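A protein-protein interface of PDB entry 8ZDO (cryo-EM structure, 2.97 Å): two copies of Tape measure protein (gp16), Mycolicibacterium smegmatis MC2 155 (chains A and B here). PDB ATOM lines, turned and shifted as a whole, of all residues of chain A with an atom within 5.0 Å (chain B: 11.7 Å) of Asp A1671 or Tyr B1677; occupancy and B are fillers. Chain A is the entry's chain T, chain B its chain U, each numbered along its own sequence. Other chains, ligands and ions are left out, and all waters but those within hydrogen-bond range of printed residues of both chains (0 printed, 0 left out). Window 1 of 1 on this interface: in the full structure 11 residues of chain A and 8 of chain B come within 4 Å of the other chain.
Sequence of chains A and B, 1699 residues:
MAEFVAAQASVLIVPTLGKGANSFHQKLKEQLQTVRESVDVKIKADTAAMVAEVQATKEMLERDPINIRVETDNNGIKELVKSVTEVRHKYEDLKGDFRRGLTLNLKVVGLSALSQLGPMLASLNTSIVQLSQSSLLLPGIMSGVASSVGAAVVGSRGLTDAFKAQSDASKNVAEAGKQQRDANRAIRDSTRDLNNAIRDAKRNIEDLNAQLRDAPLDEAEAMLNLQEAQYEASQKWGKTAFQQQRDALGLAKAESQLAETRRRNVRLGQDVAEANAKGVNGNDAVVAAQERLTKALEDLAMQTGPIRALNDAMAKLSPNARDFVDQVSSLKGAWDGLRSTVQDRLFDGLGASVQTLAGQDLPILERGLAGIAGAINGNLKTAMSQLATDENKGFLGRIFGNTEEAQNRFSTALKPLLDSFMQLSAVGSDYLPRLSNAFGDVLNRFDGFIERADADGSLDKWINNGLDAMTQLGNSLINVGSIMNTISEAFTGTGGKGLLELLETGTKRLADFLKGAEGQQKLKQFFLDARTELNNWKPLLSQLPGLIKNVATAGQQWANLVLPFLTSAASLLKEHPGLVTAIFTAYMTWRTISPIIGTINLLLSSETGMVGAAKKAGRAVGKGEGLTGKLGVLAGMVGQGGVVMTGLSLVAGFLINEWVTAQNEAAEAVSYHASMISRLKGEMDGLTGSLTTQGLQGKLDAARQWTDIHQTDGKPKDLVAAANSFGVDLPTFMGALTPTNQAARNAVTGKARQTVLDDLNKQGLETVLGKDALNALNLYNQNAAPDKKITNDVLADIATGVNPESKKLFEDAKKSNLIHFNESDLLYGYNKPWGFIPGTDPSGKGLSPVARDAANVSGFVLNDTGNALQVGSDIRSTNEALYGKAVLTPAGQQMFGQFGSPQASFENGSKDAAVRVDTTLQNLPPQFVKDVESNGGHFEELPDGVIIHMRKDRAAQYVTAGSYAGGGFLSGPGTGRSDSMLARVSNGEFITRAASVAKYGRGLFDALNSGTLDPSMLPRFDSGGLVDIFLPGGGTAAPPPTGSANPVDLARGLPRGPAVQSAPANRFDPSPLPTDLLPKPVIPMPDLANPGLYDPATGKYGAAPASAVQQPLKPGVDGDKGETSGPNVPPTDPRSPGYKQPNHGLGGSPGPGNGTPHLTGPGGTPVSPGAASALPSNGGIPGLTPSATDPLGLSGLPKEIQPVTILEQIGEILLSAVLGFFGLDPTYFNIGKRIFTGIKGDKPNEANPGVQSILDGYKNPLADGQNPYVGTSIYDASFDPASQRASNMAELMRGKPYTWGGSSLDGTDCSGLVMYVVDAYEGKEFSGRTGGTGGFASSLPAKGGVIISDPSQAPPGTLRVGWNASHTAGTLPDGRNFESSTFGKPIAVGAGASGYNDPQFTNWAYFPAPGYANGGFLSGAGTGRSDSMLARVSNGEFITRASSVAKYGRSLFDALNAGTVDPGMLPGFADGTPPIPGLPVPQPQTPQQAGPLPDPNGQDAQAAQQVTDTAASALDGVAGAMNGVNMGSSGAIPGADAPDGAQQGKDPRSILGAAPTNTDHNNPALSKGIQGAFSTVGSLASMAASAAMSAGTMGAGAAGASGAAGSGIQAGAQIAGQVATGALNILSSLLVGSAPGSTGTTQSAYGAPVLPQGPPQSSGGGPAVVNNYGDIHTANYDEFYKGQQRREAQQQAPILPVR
Along chain A the printed residues that touch a printed residue of chain B span positions 1669 to 1680.
Printed residues of chain B that touch a printed residue of chain A: Ile B1672, His B1673, Thr B1674, Ala B1675, Asn B1676, Tyr B1677, Asp B1678 and Tyr B1681.
Hydrophobic or aromatic side chains of chain B within 4 Å of the printed part of chain A: His B1673, Tyr B1677 and Tyr B1681.
Among the printed residues, 13 pairs touch across the chains.
Among the printed residues, no Asp or Glu carboxylate lies within 4 Å of a Lys or Arg side-chain nitrogen of the other chain.
Among the printed residues, merely in contact across the chains: Tyr A1669 with Thr B1674 (3.1 Å), Asp A1671 with Asn B1676 (3.4 Å), Asp A1671 with Tyr B1677 (3.7 Å), Ile A1672 with Thr B1674 (3.2 Å), His A1673 with His B1673 (3.996 Å), Asn A1676 with Tyr B1677 (3.8 Å), Tyr A1677 with Tyr B1677 (3.2 Å), Phe A1680 with Tyr B1677 (3.5 Å), Phe A1680 with Asp B1678 (3.5 Å) and Phe A1680 with Tyr B1681 (3.7 Å).
The side-chain carboxylate (OE1) of Glu B1679 lies within hydrogen-bond range of the side-chain amide nitrogen (ND2) of Asn B1676 (2.6 Å).
O of Ile A1672 sits close to O of Ile B1672, at 3.4 Å.
O of Ala B1675 sits close to OD1 of Asp A1671.
OH of Tyr B1677 lies close to O of Ala A1675, at 2.3 Å.
Asp A1671 touches Asn B1676, but with the chains exchanged Asn A1676 does not touch Asp B1671 (10.7 Å).
Ile B1672 touches its own counterpart, Ile A1672.
His A1673 touches its own counterpart, His B1673.
Ala A1675 touches Tyr B1677, but with the chains exchanged Tyr A1677 does not touch Ala B1675 (6.7 Å).
8 positions are printed for both chains.
Of the 13 pairs that touch across the chains among the printed residues, 3 have their exchanged pair printed and touching as well.
Asp A1671 touches three residues of chain B.
Tyr B1677 touches five residues of chain A.
No residue of chain B comes within 4 Å of Gly A1670.
Of chain B, only Ile B1672 (3.4 Å) and Thr B1674 (3.2 Å) come within 4 Å of Ile A1672.
Of chain B, only Tyr B1677 comes within 4 Å of Ala A1675.
Of chain B, only Tyr B1677 comes within 4 Å of Tyr A1677.
Printed residues of chain B within 4 Å of His A1673: His B1673 (3.996 Å).
Of the printed residues of chain A, Asn B1676 touches Asp A1671.
Printed residues of chain A within 4 Å of Tyr B1681: Phe A1680 (3.7 Å).
Lys B1682 touches none of the printed residues of chain A.
The nearest residue of chain B that does not touch Asp A1671 is Asp B1678 (5.3 Å).
The nearest printed residue of chain A that does not touch Tyr B1677 is His A1673 (5.0 Å).
The nearest printed residue of chain B that does not touch His A1673 is Tyr B1677 (5.0 Å).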
ATOM      1  N   TYR A1669       8.998  13.291  -5.401  1.00  0.00           N
ATOM      2  CA  TYR A1669       9.250  14.128  -6.570  1.00  0.00           C
ATOM      3  C   TYR A1669       9.395  13.269  -7.818  1.00  0.00           C
ATOM      4  O   TYR A1669       8.739  13.512  -8.838  1.00  0.00           O
ATOM      5  CB  TYR A1669      10.519  14.959  -6.364  1.00  0.00           C
ATOM      6  CG  TYR A1669      10.348  16.280  -5.651  1.00  0.00           C
ATOM      7  CD1 TYR A1669       9.965  17.419  -6.343  1.00  0.00           C
ATOM      8  CD2 TYR A1669      10.618  16.399  -4.297  1.00  0.00           C
ATOM      9  CE1 TYR A1669       9.824  18.631  -5.698  1.00  0.00           C
ATOM     10  CE2 TYR A1669      10.481  17.604  -3.644  1.00  0.00           C
ATOM     11  CZ  TYR A1669      10.084  18.718  -4.348  1.00  0.00           C
ATOM     12  OH  TYR A1669       9.946  19.922  -3.699  1.00  0.00           O
ATOM     13  N   GLY A1670      10.253  12.257  -7.750  1.00  0.00           N
ATOM     14  CA  GLY A1670      10.385  11.300  -8.829  1.00  0.00           C
ATOM     15  C   GLY A1670      11.343  11.743  -9.912  1.00  0.00           C
ATOM     16  O   GLY A1670      11.183  12.829 -10.472  1.00  0.00           O
ATOM     17  N   ASP A1671      12.343  10.905 -10.195  1.00  0.00           N
ATOM     18  CA  ASP A1671      13.352  11.082 -11.240  1.00  0.00           C
ATOM     19  C   ASP A1671      13.916  12.501 -11.327  1.00  0.00           C
ATOM     20  O   ASP A1671      14.269  12.967 -12.415  1.00  0.00           O
ATOM     21  CB  ASP A1671      12.804  10.597 -12.597  1.00  0.00           C
ATOM     22  CG  ASP A1671      11.684  11.471 -13.173  1.00  0.00           C
ATOM     23  OD1 ASP A1671      11.655  12.700 -12.969  1.00  0.00           O
ATOM     24  OD2 ASP A1671      10.805  10.898 -13.849  1.00  0.00           O
ATOM     25  N   ILE A1672      14.032  13.181 -10.188  1.00  0.00           N
ATOM     26  CA  ILE A1672      14.710  14.474 -10.143  1.00  0.00           C
ATOM     27  C   ILE A1672      16.200  14.294  -9.879  1.00  0.00           C
ATOM     28  O   ILE A1672      17.044  14.922 -10.525  1.00  0.00           O
ATOM     29  CB  ILE A1672      14.041  15.393  -9.093  1.00  0.00           C
ATOM     30  CG1 ILE A1672      14.406  15.007  -7.661  1.00  0.00           C
ATOM     31  CG2 ILE A1672      12.544  15.272  -9.193  1.00  0.00           C
ATOM     32  CD1 ILE A1672      14.062  16.061  -6.637  1.00  0.00           C
ATOM     33  N   HIS A1673      16.530  13.423  -8.935  1.00  0.00           N
ATOM     34  CA  HIS A1673      17.880  12.956  -8.675  1.00  0.00           C
ATOM     35  C   HIS A1673      18.098  11.689  -9.502  1.00  0.00           C
ATOM     36  O   HIS A1673      17.405  11.476 -10.501  1.00  0.00           O
ATOM     37  CB  HIS A1673      18.099  12.786  -7.168  1.00  0.00           C
ATOM     38  CG  HIS A1673      18.453  14.063  -6.469  1.00  0.00           C
ATOM     39  ND1 HIS A1673      18.562  14.160  -5.099  1.00  0.00           N
ATOM     40  CD2 HIS A1673      18.726  15.297  -6.956  1.00  0.00           C
ATOM     41  CE1 HIS A1673      18.887  15.399  -4.772  1.00  0.00           C
ATOM     42  NE2 HIS A1673      18.993  16.109  -5.880  1.00  0.00           N
ATOM     43  N   ALA A1675      18.708   9.275 -12.128  1.00  0.00           N
ATOM     44  CA  ALA A1675      17.962   8.536 -13.137  1.00  0.00           C
ATOM     45  C   ALA A1675      18.563   8.859 -14.499  1.00  0.00           C
ATOM     46  O   ALA A1675      18.646  10.031 -14.876  1.00  0.00           O
ATOM     47  CB  ALA A1675      16.476   8.893 -13.097  1.00  0.00           C
ATOM     48  N   ASN A1676      18.979   7.845 -15.248  1.00  0.00           N
ATOM     49  CA  ASN A1676      19.638   8.060 -16.528  1.00  0.00           C
ATOM     50  C   ASN A1676      18.687   7.827 -17.696  1.00  0.00           C
ATOM     51  O   ASN A1676      17.755   7.023 -17.619  1.00  0.00           O
ATOM     52  CB  ASN A1676      20.883   7.174 -16.658  1.00  0.00           C
ATOM     53  CG  ASN A1676      20.584   5.707 -16.452  1.00  0.00           C
ATOM     54  OD1 ASN A1676      19.441   5.322 -16.241  1.00  0.00           O
ATOM     55  ND2 ASN A1676      21.618   4.876 -16.521  1.00  0.00           N
ATOM     56  N   TYR A1677      18.930   8.565 -18.780  1.00  0.00           N
ATOM     57  CA  TYR A1677      18.027   8.567 -19.926  1.00  0.00           C
ATOM     58  C   TYR A1677      18.184   7.320 -20.781  1.00  0.00           C
ATOM     59  O   TYR A1677      17.250   6.945 -21.500  1.00  0.00           O
ATOM     60  CB  TYR A1677      18.272   9.803 -20.795  1.00  0.00           C
ATOM     61  CG  TYR A1677      18.361  11.113 -20.041  1.00  0.00           C
ATOM     62  CD1 TYR A1677      17.757  11.273 -18.803  1.00  0.00           C
ATOM     63  CD2 TYR A1677      19.062  12.190 -20.570  1.00  0.00           C
ATOM     64  CE1 TYR A1677      17.847  12.459 -18.117  1.00  0.00           C
ATOM     65  CE2 TYR A1677      19.152  13.388 -19.888  1.00  0.00           C
ATOM     66  CZ  TYR A1677      18.540  13.515 -18.660  1.00  0.00           C
ATOM     67  OH  TYR A1677      18.612  14.696 -17.962  1.00  0.00           O
ATOM     68  N   PHE A1680      15.777   4.493 -19.798  1.00  0.00           N
ATOM     69  CA  PHE A1680      14.402   4.854 -20.120  1.00  0.00           C
ATOM     70  C   PHE A1680      14.143   4.747 -21.617  1.00  0.00           C
ATOM     71  O   PHE A1680      13.111   4.208 -22.039  1.00  0.00           O
ATOM     72  CB  PHE A1680      14.097   6.264 -19.621  1.00  0.00           C
ATOM     73  CG  PHE A1680      12.706   6.727 -19.937  1.00  0.00           C
ATOM     74  CD1 PHE A1680      11.645   6.386 -19.116  1.00  0.00           C
ATOM     75  CD2 PHE A1680      12.456   7.502 -21.056  1.00  0.00           C
ATOM     76  CE1 PHE A1680      10.366   6.810 -19.408  1.00  0.00           C
ATOM     77  CE2 PHE A1680      11.180   7.925 -21.352  1.00  0.00           C
ATOM     78  CZ  PHE A1680      10.135   7.578 -20.527  1.00  0.00           C
ATOM     79  N   GLY B1670      18.203  24.544 -16.142  1.00  0.00           N
ATOM     80  CA  GLY B1670      17.207  23.858 -16.939  1.00  0.00           C
ATOM     81  C   GLY B1670      17.206  22.362 -16.723  1.00  0.00           C
ATOM     82  O   GLY B1670      18.246  21.717 -16.866  1.00  0.00           O
ATOM     83  N   ASP B1671      16.041  21.817 -16.363  1.00  0.00           N
ATOM     84  CA  ASP B1671      15.767  20.392 -16.171  1.00  0.00           C
ATOM     85  C   ASP B1671      16.894  19.630 -15.476  1.00  0.00           C
ATOM     86  O   ASP B1671      17.174  18.475 -15.817  1.00  0.00           O
ATOM     87  CB  ASP B1671      15.382  19.737 -17.513  1.00  0.00           C
ATOM     88  CG  ASP B1671      16.503  19.729 -18.549  1.00  0.00           C
ATOM     89  OD1 ASP B1671      17.696  19.647 -18.202  1.00  0.00           O
ATOM     90  OD2 ASP B1671      16.173  19.816 -19.750  1.00  0.00           O
ATOM     91  N   ILE B1672      17.527  20.255 -14.482  1.00  0.00           N
ATOM     92  CA  ILE B1672      18.522  19.551 -13.676  1.00  0.00           C
ATOM     93  C   ILE B1672      17.855  18.905 -12.466  1.00  0.00           C
ATOM     94  O   ILE B1672      18.038  17.714 -12.187  1.00  0.00           O
ATOM     95  CB  ILE B1672      19.667  20.505 -13.277  1.00  0.00           C
ATOM     96  CG1 ILE B1672      19.243  21.556 -12.258  1.00  0.00           C
ATOM     97  CG2 ILE B1672      20.106  21.296 -14.475  1.00  0.00           C
ATOM     98  CD1 ILE B1672      20.390  22.084 -11.429  1.00  0.00           C
ATOM     99  N   HIS B1673      17.058  19.681 -11.744  1.00  0.00           N
ATOM    100  CA  HIS B1673      16.135  19.203 -10.729  1.00  0.00           C
ATOM    101  C   HIS B1673      14.833  18.818 -11.430  1.00  0.00           C
ATOM    102  O   HIS B1673      14.838  18.536 -12.632  1.00  0.00           O
ATOM    103  CB  HIS B1673      15.985  20.247  -9.618  1.00  0.00           C
ATOM    104  CG  HIS B1673      17.088  20.203  -8.606  1.00  0.00           C
ATOM    105  ND1 HIS B1673      17.097  20.991  -7.475  1.00  0.00           N
ATOM    106  CD2 HIS B1673      18.214  19.453  -8.550  1.00  0.00           C
ATOM    107  CE1 HIS B1673      18.185  20.734  -6.769  1.00  0.00           C
ATOM    108  NE2 HIS B1673      18.879  19.803  -7.399  1.00  0.00           N
ATOM    109  N   THR B1674      13.724  18.776 -10.689  1.00  0.00           N
ATOM    110  CA  THR B1674      12.497  18.093 -11.080  1.00  0.00           C
ATOM    111  C   THR B1674      12.175  18.250 -12.558  1.00  0.00           C
ATOM    112  O   THR B1674      11.943  19.360 -13.047  1.00  0.00           O
ATOM    113  CB  THR B1674      11.334  18.629 -10.242  1.00  0.00           C
ATOM    114  OG1 THR B1674      11.562  18.334  -8.859  1.00  0.00           O
ATOM    115  CG2 THR B1674      10.022  17.997 -10.683  1.00  0.00           C
ATOM    116  N   ALA B1675      12.158  17.117 -13.257  1.00  0.00           N
ATOM    117  CA  ALA B1675      11.822  17.020 -14.671  1.00  0.00           C
ATOM    118  C   ALA B1675      11.661  15.547 -15.014  1.00  0.00           C
ATOM    119  O   ALA B1675      12.546  14.739 -14.714  1.00  0.00           O
ATOM    120  CB  ALA B1675      12.897  17.675 -15.540  1.00  0.00           C
ATOM    121  N   ASN B1676      10.554  15.183 -15.649  1.00  0.00           N
ATOM    122  CA  ASN B1676      10.181  13.789 -15.828  1.00  0.00           C
ATOM    123  C   ASN B1676      10.468  13.316 -17.246  1.00  0.00           C
ATOM    124  O   ASN B1676      10.436  14.095 -18.202  1.00  0.00           O
ATOM    125  CB  ASN B1676       8.701  13.584 -15.490  1.00  0.00           C
ATOM    126  CG  ASN B1676       7.813  14.646 -16.104  1.00  0.00           C
ATOM    127  OD1 ASN B1676       8.264  15.459 -16.911  1.00  0.00           O
ATOM    128  ND2 ASN B1676       6.551  14.663 -15.702  1.00  0.00           N
ATOM    129  N   TYR B1677      10.756  12.019 -17.368  1.00  0.00           N
ATOM    130  CA  TYR B1677      11.106  11.412 -18.647  1.00  0.00           C
ATOM    131  C   TYR B1677       9.878  10.971 -19.430  1.00  0.00           C
ATOM    132  O   TYR B1677       9.835  11.125 -20.654  1.00  0.00           O
ATOM    133  CB  TYR B1677      12.016  10.196 -18.435  1.00  0.00           C
ATOM    134  CG  TYR B1677      13.280  10.447 -17.643  1.00  0.00           C
ATOM    135  CD1 TYR B1677      13.746  11.734 -17.416  1.00  0.00           C
ATOM    136  CD2 TYR B1677      14.013   9.386 -17.125  1.00  0.00           C
ATOM    137  CE1 TYR B1677      14.895  11.956 -16.690  1.00  0.00           C
ATOM    138  CE2 TYR B1677      15.169   9.600 -16.402  1.00  0.00           C
ATOM    139  CZ  TYR B1677      15.605  10.889 -16.189  1.00  0.00           C
ATOM    140  OH  TYR B1677      16.753  11.121 -15.470  1.00  0.00           O
ATOM    141  N   ASP B1678       8.890  10.400 -18.738  1.00  0.00           N
ATOM    142  CA  ASP B1678       7.723   9.848 -19.414  1.00  0.00           C
ATOM    143  C   ASP B1678       6.917  10.937 -20.109  1.00  0.00           C
ATOM    144  O   ASP B1678       6.470  10.758 -21.247  1.00  0.00           O
ATOM    145  CB  ASP B1678       6.857   9.086 -18.412  1.00  0.00           C
ATOM    146  CG  ASP B1678       5.814   8.215 -19.082  1.00  0.00           C
ATOM    147  OD1 ASP B1678       6.200   7.269 -19.800  1.00  0.00           O
ATOM    148  OD2 ASP B1678       4.609   8.468 -18.878  1.00  0.00           O
ATOM    149  N   GLU B1679       6.729  12.078 -19.444  1.00  0.00           N
ATOM    150  CA  GLU B1679       5.987  13.173 -20.059  1.00  0.00           C
ATOM    151  C   GLU B1679       6.729  13.745 -21.260  1.00  0.00           C
ATOM    152  O   GLU B1679       6.110  14.056 -22.281  1.00  0.00           O
ATOM    153  CB  GLU B1679       5.703  14.262 -19.026  1.00  0.00           C
ATOM    154  CG  GLU B1679       4.418  14.037 -18.239  1.00  0.00           C
ATOM    155  CD  GLU B1679       4.543  12.941 -17.198  1.00  0.00           C
ATOM    156  OE1 GLU B1679       5.680  12.504 -16.919  1.00  0.00           O
ATOM    157  OE2 GLU B1679       3.501  12.516 -16.655  1.00  0.00           O
ATOM    158  N   PHE B1680       8.053  13.892 -21.161  1.00  0.00           N
ATOM    159  CA  PHE B1680       8.822  14.383 -22.299  1.00  0.00           C
ATOM    160  C   PHE B1680       8.736  13.423 -23.478  1.00  0.00           C
ATOM    161  O   PHE B1680       8.562  13.848 -24.629  1.00  0.00           O
ATOM    162  CB  PHE B1680      10.280  14.604 -21.895  1.00  0.00           C
ATOM    163  CG  PHE B1680      11.153  15.094 -23.016  1.00  0.00           C
ATOM    164  CD1 PHE B1680      11.263  16.448 -23.281  1.00  0.00           C
ATOM    165  CD2 PHE B1680      11.862  14.203 -23.802  1.00  0.00           C
ATOM    166  CE1 PHE B1680      12.062  16.901 -24.309  1.00  0.00           C
ATOM    167  CE2 PHE B1680      12.662  14.651 -24.833  1.00  0.00           C
ATOM    168  CZ  PHE B1680      12.762  16.002 -25.087  1.00  0.00           C
ATOM    169  N   TYR B1681       8.858  12.120 -23.210  1.00  0.00           N
ATOM    170  CA  TYR B1681       8.763  11.135 -24.281  1.00  0.00           C
ATOM    171  C   TYR B1681       7.381  11.148 -24.917  1.00  0.00           C
ATOM    172  O   TYR B1681       7.254  11.065 -26.144  1.00  0.00           O
ATOM    173  CB  TYR B1681       9.094   9.745 -23.742  1.00  0.00           C
ATOM    174  CG  TYR B1681       9.283   8.704 -24.818  1.00  0.00           C
ATOM    175  CD1 TYR B1681      10.491   8.583 -25.488  1.00  0.00           C
ATOM    176  CD2 TYR B1681       8.253   7.840 -25.162  1.00  0.00           C
ATOM    177  CE1 TYR B1681      10.667   7.636 -26.473  1.00  0.00           C
ATOM    178  CE2 TYR B1681       8.422   6.889 -26.146  1.00  0.00           C
ATOM    179  CZ  TYR B1681       9.630   6.790 -26.798  1.00  0.00           C
ATOM    180  OH  TYR B1681       9.802   5.841 -27.779  1.00  0.00           O
ATOM    181  N   LYS B1682       6.332  11.257 -24.100  1.00  0.00           N
ATOM    182  CA  LYS B1682       4.980  11.306 -24.643  1.00  0.00           C
ATOM    183  C   LYS B1682       4.758  12.569 -25.464  1.00  0.00           C
ATOM    184  O   LYS B1682       4.070  12.534 -26.488  1.00  0.00           O
ATOM    185  CB  LYS B1682       3.955  11.202 -23.516  1.00  0.00           C
ATOM    186  CG  LYS B1682       3.707   9.778 -23.050  1.00  0.00           C
ATOM    187  CD  LYS B1682       2.443   9.677 -22.214  1.00  0.00           C
ATOM    188  CE  LYS B1682       2.694  10.099 -20.779  1.00  0.00           C
ATOM    189  NZ  LYS B1682       1.492  10.717 -20.159  1.00  0.00           N
ATOM    190  N   GLY B1683       5.329  13.694 -25.034  1.00  0.00           N
ATOM    191  CA  GLY B1683       5.214  14.912 -25.819  1.00  0.00           C
ATOM    192  C   GLY B1683       5.915  14.810 -27.160  1.00  0.00           C
ATOM    193  O   GLY B1683       5.385  15.254 -28.184  1.00  0.00           O
ATOM    194  N   GLN B1684       7.114  14.227 -27.174  1.00  0.00           N
ATOM    195  CA  GLN B1684       7.811  14.017 -28.439  1.00  0.00           C
ATOM    196  C   GLN B1684       7.030  13.077 -29.347  1.00  0.00           C
ATOM    197  O   GLN B1684       6.933  13.304 -30.560  1.00  0.00           O
ATOM    198  CB  GLN B1684       9.216  13.477 -28.183  1.00  0.00           C
ATOM    199  CG  GLN B1684      10.183  14.507 -27.627  1.00  0.00           C
ATOM    200  CD  GLN B1684      10.194  15.794 -28.430  1.00  0.00           C
ATOM    201  OE1 GLN B1684      10.078  16.886 -27.874  1.00  0.00           O
ATOM    202  NE2 GLN B1684      10.337  15.672 -29.744  1.00  0.00           N
ATOM    203  N   GLN B1685       6.459  12.015 -28.773  1.00  0.00           N
ATOM    204  CA  GLN B1685       5.641  11.100 -29.560  1.00  0.00           C
ATOM    205  C   GLN B1685       4.412  11.803 -30.119  1.00  0.00           C
ATOM    206  O   GLN B1685       4.010  11.548 -31.256  1.00  0.00           O
ATOM    207  CB  GLN B1685       5.231   9.896 -28.713  1.00  0.00           C
ATOM    208  CG  GLN B1685       6.367   8.938 -28.397  1.00  0.00           C
ATOM    209  CD  GLN B1685       7.370   8.828 -29.524  1.00  0.00           C
ATOM    210  OE1 GLN B1685       7.113   8.177 -30.536  1.00  0.00           O
ATOM    211  NE2 GLN B1685       8.524   9.462 -29.354  1.00  0.00           N
ATOM    212  N   ARG B1686       3.801  12.692 -29.333  1.00  0.00           N
ATOM    213  CA  ARG B1686       2.638  13.431 -29.812  1.00  0.00           C
ATOM    214  C   ARG B1686       3.009  14.375 -30.947  1.00  0.00           C
ATOM    215  O   ARG B1686       2.256  14.510 -31.917  1.00  0.00           O
ATOM    216  CB  ARG B1686       1.995  14.203 -28.661  1.00  0.00           C
ATOM    217  CG  ARG B1686       0.696  13.596 -28.164  1.00  0.00           C
ATOM    218  CD  ARG B1686       0.157  14.354 -26.964  1.00  0.00           C
ATOM    219  NE  ARG B1686       1.017  14.214 -25.794  1.00  0.00           N
ATOM    220  CZ  ARG B1686       1.570  15.230 -25.147  1.00  0.00           C
ATOM    221  NH1 ARG B1686       1.382  16.480 -25.533  1.00  0.00           N
ATOM    222  NH2 ARG B1686       2.329  14.984 -24.083  1.00  0.00           N
